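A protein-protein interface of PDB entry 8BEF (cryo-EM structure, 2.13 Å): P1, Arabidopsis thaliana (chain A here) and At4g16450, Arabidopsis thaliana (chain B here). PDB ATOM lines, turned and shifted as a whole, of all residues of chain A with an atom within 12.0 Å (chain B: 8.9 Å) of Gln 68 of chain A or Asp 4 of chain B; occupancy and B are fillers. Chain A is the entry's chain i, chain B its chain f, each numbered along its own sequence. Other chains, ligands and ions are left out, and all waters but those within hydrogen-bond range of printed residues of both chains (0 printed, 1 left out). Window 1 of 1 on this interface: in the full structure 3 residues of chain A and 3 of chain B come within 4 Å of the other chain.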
ATOM      1  N   GLU A  57     -11.752  22.967   7.900  1.00  0.00           N
ATOM      2  CA  GLU A  57     -10.609  22.100   7.629  1.00  0.00           C
ATOM      3  C   GLU A  57     -11.013  20.809   6.933  1.00  0.00           C
ATOM      4  O   GLU A  57     -10.254  20.291   6.106  1.00  0.00           O
ATOM      5  CB  GLU A  57      -9.872  21.788   8.932  1.00  0.00           C
ATOM      6  CG  GLU A  57      -8.954  22.903   9.405  1.00  0.00           C
ATOM      7  CD  GLU A  57      -9.714  24.077   9.994  1.00  0.00           C
ATOM      8  OE1 GLU A  57     -10.901  23.906  10.343  1.00  0.00           O
ATOM      9  OE2 GLU A  57      -9.124  25.173  10.107  1.00  0.00           O
ATOM     10  N   ARG A  58     -12.195  20.272   7.250  1.00  0.00           N
ATOM     11  CA  ARG A  58     -12.659  19.058   6.587  1.00  0.00           C
ATOM     12  C   ARG A  58     -12.714  19.230   5.073  1.00  0.00           C
ATOM     13  O   ARG A  58     -12.534  18.260   4.329  1.00  0.00           O
ATOM     14  CB  ARG A  58     -14.031  18.656   7.131  1.00  0.00           C
ATOM     15  CG  ARG A  58     -14.745  17.572   6.334  1.00  0.00           C
ATOM     16  CD  ARG A  58     -14.053  16.225   6.486  1.00  0.00           C
ATOM     17  NE  ARG A  58     -13.023  16.004   5.478  1.00  0.00           N
ATOM     18  CZ  ARG A  58     -12.169  14.988   5.491  1.00  0.00           C
ATOM     19  NH1 ARG A  58     -12.199  14.073   6.444  1.00  0.00           N
ATOM     20  NH2 ARG A  58     -11.263  14.889   4.523  1.00  0.00           N
ATOM     21  N   ASN A  60     -10.677  21.203   3.213  1.00  0.00           N
ATOM     22  CA  ASN A  60      -9.381  21.553   2.644  1.00  0.00           C
ATOM     23  C   ASN A  60      -8.457  20.340   2.590  1.00  0.00           C
ATOM     24  O   ASN A  60      -7.247  20.451   2.789  1.00  0.00           O
ATOM     25  CB  ASN A  60      -8.731  22.687   3.431  1.00  0.00           C
ATOM     26  CG  ASN A  60      -9.445  24.013   3.244  1.00  0.00           C
ATOM     27  OD1 ASN A  60     -10.129  24.230   2.244  1.00  0.00           O
ATOM     28  ND2 ASN A  60      -9.286  24.910   4.213  1.00  0.00           N
ATOM     29  N   ALA A  61      -9.029  19.164   2.325  1.00  0.00           N
ATOM     30  CA  ALA A  61      -8.238  17.937   2.336  1.00  0.00           C
ATOM     31  C   ALA A  61      -7.139  17.967   1.278  1.00  0.00           C
ATOM     32  O   ALA A  61      -6.003  17.566   1.550  1.00  0.00           O
ATOM     33  CB  ALA A  61      -9.148  16.725   2.134  1.00  0.00           C
ATOM     34  N   GLN A  62      -7.452  18.444   0.070  1.00  0.00           N
ATOM     35  CA  GLN A  62      -6.462  18.416  -1.003  1.00  0.00           C
ATOM     36  C   GLN A  62      -5.297  19.360  -0.713  1.00  0.00           C
ATOM     37  O   GLN A  62      -4.148  19.051  -1.043  1.00  0.00           O
ATOM     38  CB  GLN A  62      -7.121  18.749  -2.346  1.00  0.00           C
ATOM     39  CG  GLN A  62      -6.136  19.046  -3.475  1.00  0.00           C
ATOM     40  CD  GLN A  62      -6.803  19.216  -4.835  1.00  0.00           C
ATOM     41  OE1 GLN A  62      -7.898  19.763  -4.942  1.00  0.00           O
ATOM     42  NE2 GLN A  62      -6.133  18.750  -5.881  1.00  0.00           N
ATOM     43  N   LEU A  63      -5.572  20.505  -0.084  1.00  0.00           N
ATOM     44  CA  LEU A  63      -4.508  21.442   0.266  1.00  0.00           C
ATOM     45  C   LEU A  63      -3.472  20.832   1.200  1.00  0.00           C
ATOM     46  O   LEU A  63      -2.332  21.302   1.230  1.00  0.00           O
ATOM     47  CB  LEU A  63      -5.098  22.698   0.909  1.00  0.00           C
ATOM     48  CG  LEU A  63      -5.774  23.721  -0.009  1.00  0.00           C
ATOM     49  CD1 LEU A  63      -5.804  25.075   0.659  1.00  0.00           C
ATOM     50  CD2 LEU A  63      -5.074  23.808  -1.350  1.00  0.00           C
ATOM     51  N   ARG A  64      -3.835  19.802   1.965  1.00  0.00           N
ATOM     52  CA  ARG A  64      -2.897  19.162   2.877  1.00  0.00           C
ATOM     53  C   ARG A  64      -2.357  17.837   2.360  1.00  0.00           C
ATOM     54  O   ARG A  64      -1.266  17.432   2.773  1.00  0.00           O
ATOM     55  CB  ARG A  64      -3.554  18.935   4.241  1.00  0.00           C
ATOM     56  CG  ARG A  64      -4.422  20.087   4.698  1.00  0.00           C
ATOM     57  CD  ARG A  64      -4.413  20.210   6.210  1.00  0.00           C
ATOM     58  NE  ARG A  64      -5.055  19.074   6.862  1.00  0.00           N
ATOM     59  CZ  ARG A  64      -6.356  18.824   6.829  1.00  0.00           C
ATOM     60  NH1 ARG A  64      -7.197  19.607   6.173  1.00  0.00           N
ATOM     61  NH2 ARG A  64      -6.828  17.761   7.472  1.00  0.00           N
ATOM     62  N   TRP A  65      -3.089  17.158   1.477  1.00  0.00           N
ATOM     63  CA  TRP A  65      -2.625  15.884   0.940  1.00  0.00           C
ATOM     64  C   TRP A  65      -1.666  16.090  -0.225  1.00  0.00           C
ATOM     65  O   TRP A  65      -0.574  15.520  -0.244  1.00  0.00           O
ATOM     66  CB  TRP A  65      -3.819  15.034   0.505  1.00  0.00           C
ATOM     67  CG  TRP A  65      -3.437  13.770  -0.196  1.00  0.00           C
ATOM     68  CD1 TRP A  65      -3.678  13.450  -1.499  1.00  0.00           C
ATOM     69  CD2 TRP A  65      -2.761  12.644   0.373  1.00  0.00           C
ATOM     70  NE1 TRP A  65      -3.185  12.202  -1.782  1.00  0.00           N
ATOM     71  CE2 TRP A  65      -2.618  11.683  -0.649  1.00  0.00           C
ATOM     72  CE3 TRP A  65      -2.253  12.358   1.642  1.00  0.00           C
ATOM     73  CZ2 TRP A  65      -1.990  10.459  -0.438  1.00  0.00           C
ATOM     74  CZ3 TRP A  65      -1.632  11.139   1.850  1.00  0.00           C
ATOM     75  CH2 TRP A  65      -1.506  10.206   0.816  1.00  0.00           C
ATOM     76  N   ASP A  66      -2.061  16.913  -1.193  1.00  0.00           N
ATOM     77  CA  ASP A  66      -1.270  17.093  -2.408  1.00  0.00           C
ATOM     78  C   ASP A  66       0.181  17.500  -2.162  1.00  0.00           C
ATOM     79  O   ASP A  66       1.054  17.014  -2.901  1.00  0.00           O
ATOM     80  CB  ASP A  66      -1.973  18.103  -3.329  1.00  0.00           C
ATOM     81  CG  ASP A  66      -3.006  17.444  -4.235  1.00  0.00           C
ATOM     82  OD1 ASP A  66      -3.319  16.257  -4.016  1.00  0.00           O
ATOM     83  OD2 ASP A  66      -3.503  18.109  -5.165  1.00  0.00           O
ATOM     84  N   PRO A  67       0.517  18.368  -1.197  1.00  0.00           N
ATOM     85  CA  PRO A  67       1.945  18.617  -0.936  1.00  0.00           C
ATOM     86  C   PRO A  67       2.718  17.364  -0.562  1.00  0.00           C
ATOM     87  O   PRO A  67       3.921  17.290  -0.835  1.00  0.00           O
ATOM     88  CB  PRO A  67       1.936  19.635   0.215  1.00  0.00           C
ATOM     89  CG  PRO A  67       0.597  20.261   0.188  1.00  0.00           C
ATOM     90  CD  PRO A  67      -0.355  19.317  -0.481  1.00  0.00           C
ATOM     91  N   GLN A  68       2.063  16.372   0.050  1.00  0.00           N
ATOM     92  CA  GLN A  68       2.756  15.149   0.438  1.00  0.00           C
ATOM     93  C   GLN A  68       3.111  14.271  -0.760  1.00  0.00           C
ATOM     94  O   GLN A  68       4.017  13.439  -0.650  1.00  0.00           O
ATOM     95  CB  GLN A  68       1.907  14.353   1.437  1.00  0.00           C
ATOM     96  CG  GLN A  68       1.762  15.005   2.809  1.00  0.00           C
ATOM     97  CD  GLN A  68       0.793  14.257   3.712  1.00  0.00           C
ATOM     98  OE1 GLN A  68       0.999  13.087   4.027  1.00  0.00           O
ATOM     99  NE2 GLN A  68      -0.276  14.928   4.123  1.00  0.00           N
ATOM    100  N   ILE A  69       2.420  14.424  -1.888  1.00  0.00           N
ATOM    101  CA  ILE A  69       2.708  13.669  -3.103  1.00  0.00           C
ATOM    102  C   ILE A  69       3.310  14.552  -4.189  1.00  0.00           C
ATOM    103  O   ILE A  69       3.347  14.150  -5.355  1.00  0.00           O
ATOM    104  CB  ILE A  69       1.458  12.946  -3.634  1.00  0.00           C
ATOM    105  CG1 ILE A  69       0.286  13.925  -3.767  1.00  0.00           C
ATOM    106  CG2 ILE A  69       1.118  11.741  -2.762  1.00  0.00           C
ATOM    107  CD1 ILE A  69      -0.841  13.427  -4.646  1.00  0.00           C
ATOM    108  N   SER A  70       3.787  15.746  -3.835  1.00  0.00           N
ATOM    109  CA  SER A  70       4.242  16.702  -4.837  1.00  0.00           C
ATOM    110  C   SER A  70       5.512  16.254  -5.552  1.00  0.00           C
ATOM    111  O   SER A  70       5.820  16.783  -6.623  1.00  0.00           O
ATOM    112  CB  SER A  70       4.459  18.073  -4.188  1.00  0.00           C
ATOM    113  OG  SER A  70       5.570  18.053  -3.315  1.00  0.00           O
ATOM    114  N   GLN A  71       6.250  15.301  -4.991  1.00  0.00           N
ATOM    115  CA  GLN A  71       7.466  14.785  -5.602  1.00  0.00           C
ATOM    116  C   GLN A  71       7.248  13.447  -6.300  1.00  0.00           C
ATOM    117  O   GLN A  71       8.221  12.789  -6.673  1.00  0.00           O
ATOM    118  CB  GLN A  71       8.568  14.653  -4.548  1.00  0.00           C
ATOM    119  CG  GLN A  71       9.421  15.900  -4.365  1.00  0.00           C
ATOM    120  CD  GLN A  71       8.664  17.178  -4.663  1.00  0.00           C
ATOM    121  OE1 GLN A  71       7.786  17.586  -3.906  1.00  0.00           O
ATOM    122  NE2 GLN A  71       8.998  17.813  -5.778  1.00  0.00           N
ATOM    123  N   VAL A  72       5.997  13.035  -6.480  1.00  0.00           N
ATOM    124  CA  VAL A  72       5.691  11.726  -7.047  1.00  0.00           C
ATOM    125  C   VAL A  72       5.754  11.804  -8.566  1.00  0.00           C
ATOM    126  O   VAL A  72       5.201  12.726  -9.177  1.00  0.00           O
ATOM    127  CB  VAL A  72       4.312  11.243  -6.568  1.00  0.00           C
ATOM    128  CG1 VAL A  72       3.841  10.055  -7.392  1.00  0.00           C
ATOM    129  CG2 VAL A  72       4.358  10.898  -5.087  1.00  0.00           C
ATOM    130  N   ALA A  73       6.430  10.834  -9.178  1.00  0.00           N
ATOM    131  CA  ALA A  73       6.515  10.778 -10.631  1.00  0.00           C
ATOM    132  C   ALA A  73       5.121  10.682 -11.240  1.00  0.00           C
ATOM    133  O   ALA A  73       4.308   9.845 -10.839  1.00  0.00           O
ATOM    134  CB  ALA A  73       7.373   9.591 -11.065  1.00  0.00           C
ATOM    135  N   GLY A  74       4.852  11.547 -12.212  1.00  0.00           N
ATOM    136  CA  GLY A  74       3.545  11.688 -12.810  1.00  0.00           C
ATOM    137  C   GLY A  74       2.887  13.027 -12.555  1.00  0.00           C
ATOM    138  O   GLY A  74       1.941  13.381 -13.268  1.00  0.00           O
ATOM    139  N   ARG A  75       3.363  13.790 -11.562  1.00  0.00           N
ATOM    140  CA  ARG A  75       2.779  15.096 -11.283  1.00  0.00           C
ATOM    141  C   ARG A  75       3.836  16.148 -10.950  1.00  0.00           C
ATOM    142  O   ARG A  75       3.496  17.201 -10.402  1.00  0.00           O
ATOM    143  CB  ARG A  75       1.755  15.003 -10.142  1.00  0.00           C
ATOM    144  CG  ARG A  75       2.329  14.544  -8.815  1.00  0.00           C
ATOM    145  CD  ARG A  75       1.226  14.158  -7.842  1.00  0.00           C
ATOM    146  NE  ARG A  75       0.481  15.313  -7.359  1.00  0.00           N
ATOM    147  CZ  ARG A  75      -0.758  15.612  -7.724  1.00  0.00           C
ATOM    148  NH1 ARG A  75      -1.425  14.861  -8.586  1.00  0.00           N
ATOM    149  NH2 ARG A  75      -1.341  16.691  -7.213  1.00  0.00           N
ATOM    150  N   ARG A  76       5.097  15.898 -11.277  1.00  0.00           N
ATOM    151  CA  ARG A  76       6.174  16.834 -10.995  1.00  0.00           C
ATOM    152  C   ARG A  76       6.331  17.848 -12.119  1.00  0.00           C
ATOM    153  O   ARG A  76       6.055  17.562 -13.287  1.00  0.00           O
ATOM    154  CB  ARG A  76       7.490  16.085 -10.795  1.00  0.00           C
ATOM    155  CG  ARG A  76       7.376  14.918  -9.846  1.00  0.00           C
ATOM    156  CD  ARG A  76       8.729  14.383  -9.467  1.00  0.00           C
ATOM    157  NE  ARG A  76       9.487  15.341  -8.673  1.00  0.00           N
ATOM    158  CZ  ARG A  76      10.797  15.280  -8.485  1.00  0.00           C
ATOM    159  NH1 ARG A  76      11.523  14.309  -9.010  1.00  0.00           N
ATOM    160  NH2 ARG A  76      11.391  16.217  -7.754  1.00  0.00           N
ATOM    161  N   ASP A  80      12.035  19.896 -12.179  1.00  0.00           N
ATOM    162  CA  ASP A  80      12.498  19.283 -10.935  1.00  0.00           C
ATOM    163  C   ASP A  80      13.456  18.129 -11.191  1.00  0.00           C
ATOM    164  O   ASP A  80      14.389  17.912 -10.411  1.00  0.00           O
ATOM    165  CB  ASP A  80      11.308  18.800 -10.106  1.00  0.00           C
ATOM    166  CG  ASP A  80      10.183  19.801 -10.071  1.00  0.00           C
ATOM    167  OD1 ASP A  80      10.444  20.983 -10.362  1.00  0.00           O
ATOM    168  OD2 ASP A  80       9.039  19.410  -9.765  1.00  0.00           O
ATOM    169  N   FME B   1       4.415   4.583  -1.953  1.00  0.00           N
ATOM    170  CN  FME B   1       5.386   4.063  -1.135  1.00  0.00           C
ATOM    171  O1  FME B   1       6.488   3.680  -1.543  1.00  0.00           O
ATOM    172  CA  FME B   1       3.136   5.024  -1.475  1.00  0.00           C
ATOM    173  CB  FME B   1       2.199   3.852  -1.116  1.00  0.00           C
ATOM    174  CG  FME B   1       1.480   3.321  -2.327  1.00  0.00           C
ATOM    175  SD  FME B   1      -0.197   3.883  -2.238  1.00  0.00           S
ATOM    176  CE  FME B   1      -0.193   5.227  -3.360  1.00  0.00           C
ATOM    177  C   FME B   1       3.237   5.904  -0.234  1.00  0.00           C
ATOM    178  O   FME B   1       3.377   5.248   0.948  1.00  0.00           O
ATOM    179  N   ASN B   2       2.869   7.170  -0.384  1.00  0.00           N
ATOM    180  CA  ASN B   2       2.799   8.077   0.751  1.00  0.00           C
ATOM    181  C   ASN B   2       1.589   7.729   1.605  1.00  0.00           C
ATOM    182  O   ASN B   2       0.498   7.501   1.085  1.00  0.00           O
ATOM    183  CB  ASN B   2       2.718   9.528   0.286  1.00  0.00           C
ATOM    184  CG  ASN B   2       3.256  10.498   1.316  1.00  0.00           C
ATOM    185  OD1 ASN B   2       2.528  10.948   2.200  1.00  0.00           O
ATOM    186  ND2 ASN B   2       4.539  10.824   1.210  1.00  0.00           N
ATOM    187  N   THR B   3       1.783   7.696   2.917  1.00  0.00           N
ATOM    188  CA  THR B   3       0.719   7.362   3.849  1.00  0.00           C
ATOM    189  C   THR B   3       0.581   8.473   4.880  1.00  0.00           C
ATOM    190  O   THR B   3       1.507   9.252   5.114  1.00  0.00           O
ATOM    191  CB  THR B   3       0.982   6.018   4.543  1.00  0.00           C
ATOM    192  OG1 THR B   3       2.190   6.101   5.305  1.00  0.00           O
ATOM    193  CG2 THR B   3       1.120   4.907   3.515  1.00  0.00           C
ATOM    194  N   ASP B   4      -0.604   8.545   5.485  1.00  0.00           N
ATOM    195  CA  ASP B   4      -0.885   9.542   6.518  1.00  0.00           C
ATOM    196  C   ASP B   4      -2.016   9.005   7.384  1.00  0.00           C
ATOM    197  O   ASP B   4      -3.170   8.995   6.950  1.00  0.00           O
ATOM    198  CB  ASP B   4      -1.257  10.883   5.898  1.00  0.00           C
ATOM    199  CG  ASP B   4      -1.155  12.031   6.885  1.00  0.00           C
ATOM    200  OD1 ASP B   4      -1.015  11.766   8.097  1.00  0.00           O
ATOM    201  OD2 ASP B   4      -1.226  13.201   6.451  1.00  0.00           O
ATOM    202  N   ILE B   5      -1.687   8.581   8.606  1.00  0.00           N
ATOM    203  CA  ILE B   5      -2.683   8.012   9.510  1.00  0.00           C
ATOM    204  C   ILE B   5      -3.612   9.058  10.105  1.00  0.00           C
ATOM    205  O   ILE B   5      -4.652   8.698  10.664  1.00  0.00           O
ATOM    206  CB  ILE B   5      -1.981   7.227  10.637  1.00  0.00           C
ATOM    207  CG1 ILE B   5      -2.933   6.208  11.275  1.00  0.00           C
ATOM    208  CG2 ILE B   5      -1.445   8.178  11.698  1.00  0.00           C
ATOM    209  CD1 ILE B   5      -3.374   5.109  10.345  1.00  0.00           C
ATOM    210  N   THR B   6      -3.272  10.339   9.977  1.00  0.00           N
ATOM    211  CA  THR B   6      -3.963  11.416  10.677  1.00  0.00           C
ATOM    212  C   THR B   6      -5.468  11.371  10.444  1.00  0.00           C
ATOM    213  O   THR B   6      -5.935  11.387   9.303  1.00  0.00           O
ATOM    214  CB  THR B   6      -3.396  12.764  10.224  1.00  0.00           C
ATOM    215  OG1 THR B   6      -2.042  12.881  10.671  1.00  0.00           O
ATOM    216  CG2 THR B   6      -4.214  13.910  10.790  1.00  0.00           C
ATOM    217  N   ALA B   7      -6.222  11.316  11.535  1.00  0.00           N
ATOM    218  CA  ALA B   7      -7.670  11.206  11.479  1.00  0.00           C
ATOM    219  C   ALA B   7      -8.314  12.586  11.439  1.00  0.00           C
ATOM    220  O   ALA B   7      -7.704  13.597  11.789  1.00  0.00           O
ATOM    221  CB  ALA B   7      -8.201  10.417  12.676  1.00  0.00           C
ATOM    222  N   LEU B   8      -9.569  12.612  10.992  1.00  0.00           N
ATOM    223  CA  LEU B   8     -10.313  13.865  10.958  1.00  0.00           C
ATOM    224  C   LEU B   8     -10.657  14.335  12.367  1.00  0.00           C
ATOM    225  O   LEU B   8     -10.449  15.503  12.710  1.00  0.00           O
ATOM    226  CB  LEU B   8     -11.575  13.695  10.113  1.00  0.00           C
ATOM    227  CG  LEU B   8     -12.647  14.773  10.254  1.00  0.00           C
ATOM    228  CD1 LEU B   8     -12.168  16.071   9.636  1.00  0.00           C
ATOM    229  CD2 LEU B   8     -13.945  14.315   9.613  1.00  0.00           C
ATOM    230  N   LYS B  10      -9.780  14.196  16.223  1.00  0.00           N
ATOM    231  CA  LYS B  10      -8.609  13.905  17.034  1.00  0.00           C
ATOM    232  C   LYS B  10      -8.954  12.959  18.182  1.00  0.00           C
ATOM    233  O   LYS B  10     -10.100  12.861  18.626  1.00  0.00           O
ATOM    234  CB  LYS B  10      -8.010  15.198  17.587  1.00  0.00           C
ATOM    235  CG  LYS B  10      -6.802  15.710  16.818  1.00  0.00           C
ATOM    236  CD  LYS B  10      -7.092  15.836  15.332  1.00  0.00           C
ATOM    237  CE  LYS B  10      -5.840  16.207  14.556  1.00  0.00           C
ATOM    238  NZ  LYS B  10      -6.034  16.060  13.087  1.00  0.00           N
ATOM    239  N   ARG B  18       1.034   6.337  18.000  1.00  0.00           N
ATOM    240  CA  ARG B  18       0.247   6.953  16.936  1.00  0.00           C
ATOM    241  C   ARG B  18      -0.150   5.943  15.865  1.00  0.00           C
ATOM    242  O   ARG B  18      -1.298   5.932  15.408  1.00  0.00           O
ATOM    243  CB  ARG B  18       1.036   8.108  16.318  1.00  0.00           C
ATOM    244  CG  ARG B  18       0.185   9.264  15.836  1.00  0.00           C
ATOM    245  CD  ARG B  18       1.051  10.397  15.307  1.00  0.00           C
ATOM    246  NE  ARG B  18       1.307  10.276  13.877  1.00  0.00           N
ATOM    247  CZ  ARG B  18       0.532  10.780  12.926  1.00  0.00           C
ATOM    248  NH1 ARG B  18      -0.573  11.448  13.214  1.00  0.00           N
ATOM    249  NH2 ARG B  18       0.870  10.603  11.654  1.00  0.00           N
ATOM    250  N   ASN B  19       0.786   5.094  15.445  1.00  0.00           N
ATOM    251  CA  ASN B  19       0.552   4.108  14.388  1.00  0.00           C
ATOM    252  C   ASN B  19       1.135   2.771  14.827  1.00  0.00           C
ATOM    253  O   ASN B  19       2.194   2.349  14.352  1.00  0.00           O
ATOM    254  CB  ASN B  19       1.165   4.577  13.065  1.00  0.00           C
ATOM    255  CG  ASN B  19       0.609   3.838  11.861  1.00  0.00           C
ATOM    256  OD1 ASN B  19       0.192   2.684  11.960  1.00  0.00           O
ATOM    257  ND2 ASN B  19       0.602   4.502  10.715  1.00  0.00           N
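OD1 of Asn 2 of chain B lies close to OE1 of Gln 68 of chain A (3.2 Å). The side-chain carboxylate (OD2) of Asp 4 of chain B lies within hydrogen-bond range of the side-chain amide nitrogen (NE2) of Gln 68 of chain A (3.1 Å).
NE2 of Gln 68 of chain A is in hydrogen-bond range of O of Arg 64 of chain A (3.0 Å). The side-chain hydroxyl (OG1) of Thr 6 of chain B sits at hydrogen-bond distance from the side-chain carboxylate (OD1) of Asp 4 of chain B (3.0 Å).
Among the printed residues, merely in contact across the chains: Arg 58 of chain A with Leu 8 of chain B (3.6 Å) and Trp 65 of chain A with Asn 2 of chain B (3.4 Å).
Asp 4 of chain B touches one residue of chain A. No residue of chain B comes within 4 Å of Pro 67 of chain A. Thr 6 of chain B touches none of the printed residues of chain A. No residue of chain A comes within 4 Å of Ala 7 of chain B. Printed residues of chain B within 4 Å of Trp 65 of chain A: Asn 2. Printed residues of chain A within 4 Å of Leu 8 of chain B: Arg 58 (3.6 Å). Printed residues of chain B within 4 Å of Arg 58 of chain A: Leu 8. Gly 74 of chain A touches none of the printed residues of chain B. Ala 61 of chain A touches none of the printed residues of chain B. The nearest residue of chain A that does not touch Asp 4 of chain B is Trp 65 of chain A (4.1 Å). The nearest printed residue of chain A that does not touch Leu 8 of chain B is Glu 57 of chain A (5.6 Å).
Hydrophobic or aromatic side chains of chain B within 4 Å of the printed part of chain A: Leu 8. Along chain B the printed residues that touch a printed residue of chain A span positions 2 to 8. Hydrophobic or aromatic side chains of chain A within 4 Å of the printed part of chain B: Trp 65. Among the printed residues, 4 pairs touch across the chains. Among the printed residues, no Asp or Glu carboxylate lies within 4 Å of a Lys or Arg side-chain nitrogen of the other chain.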
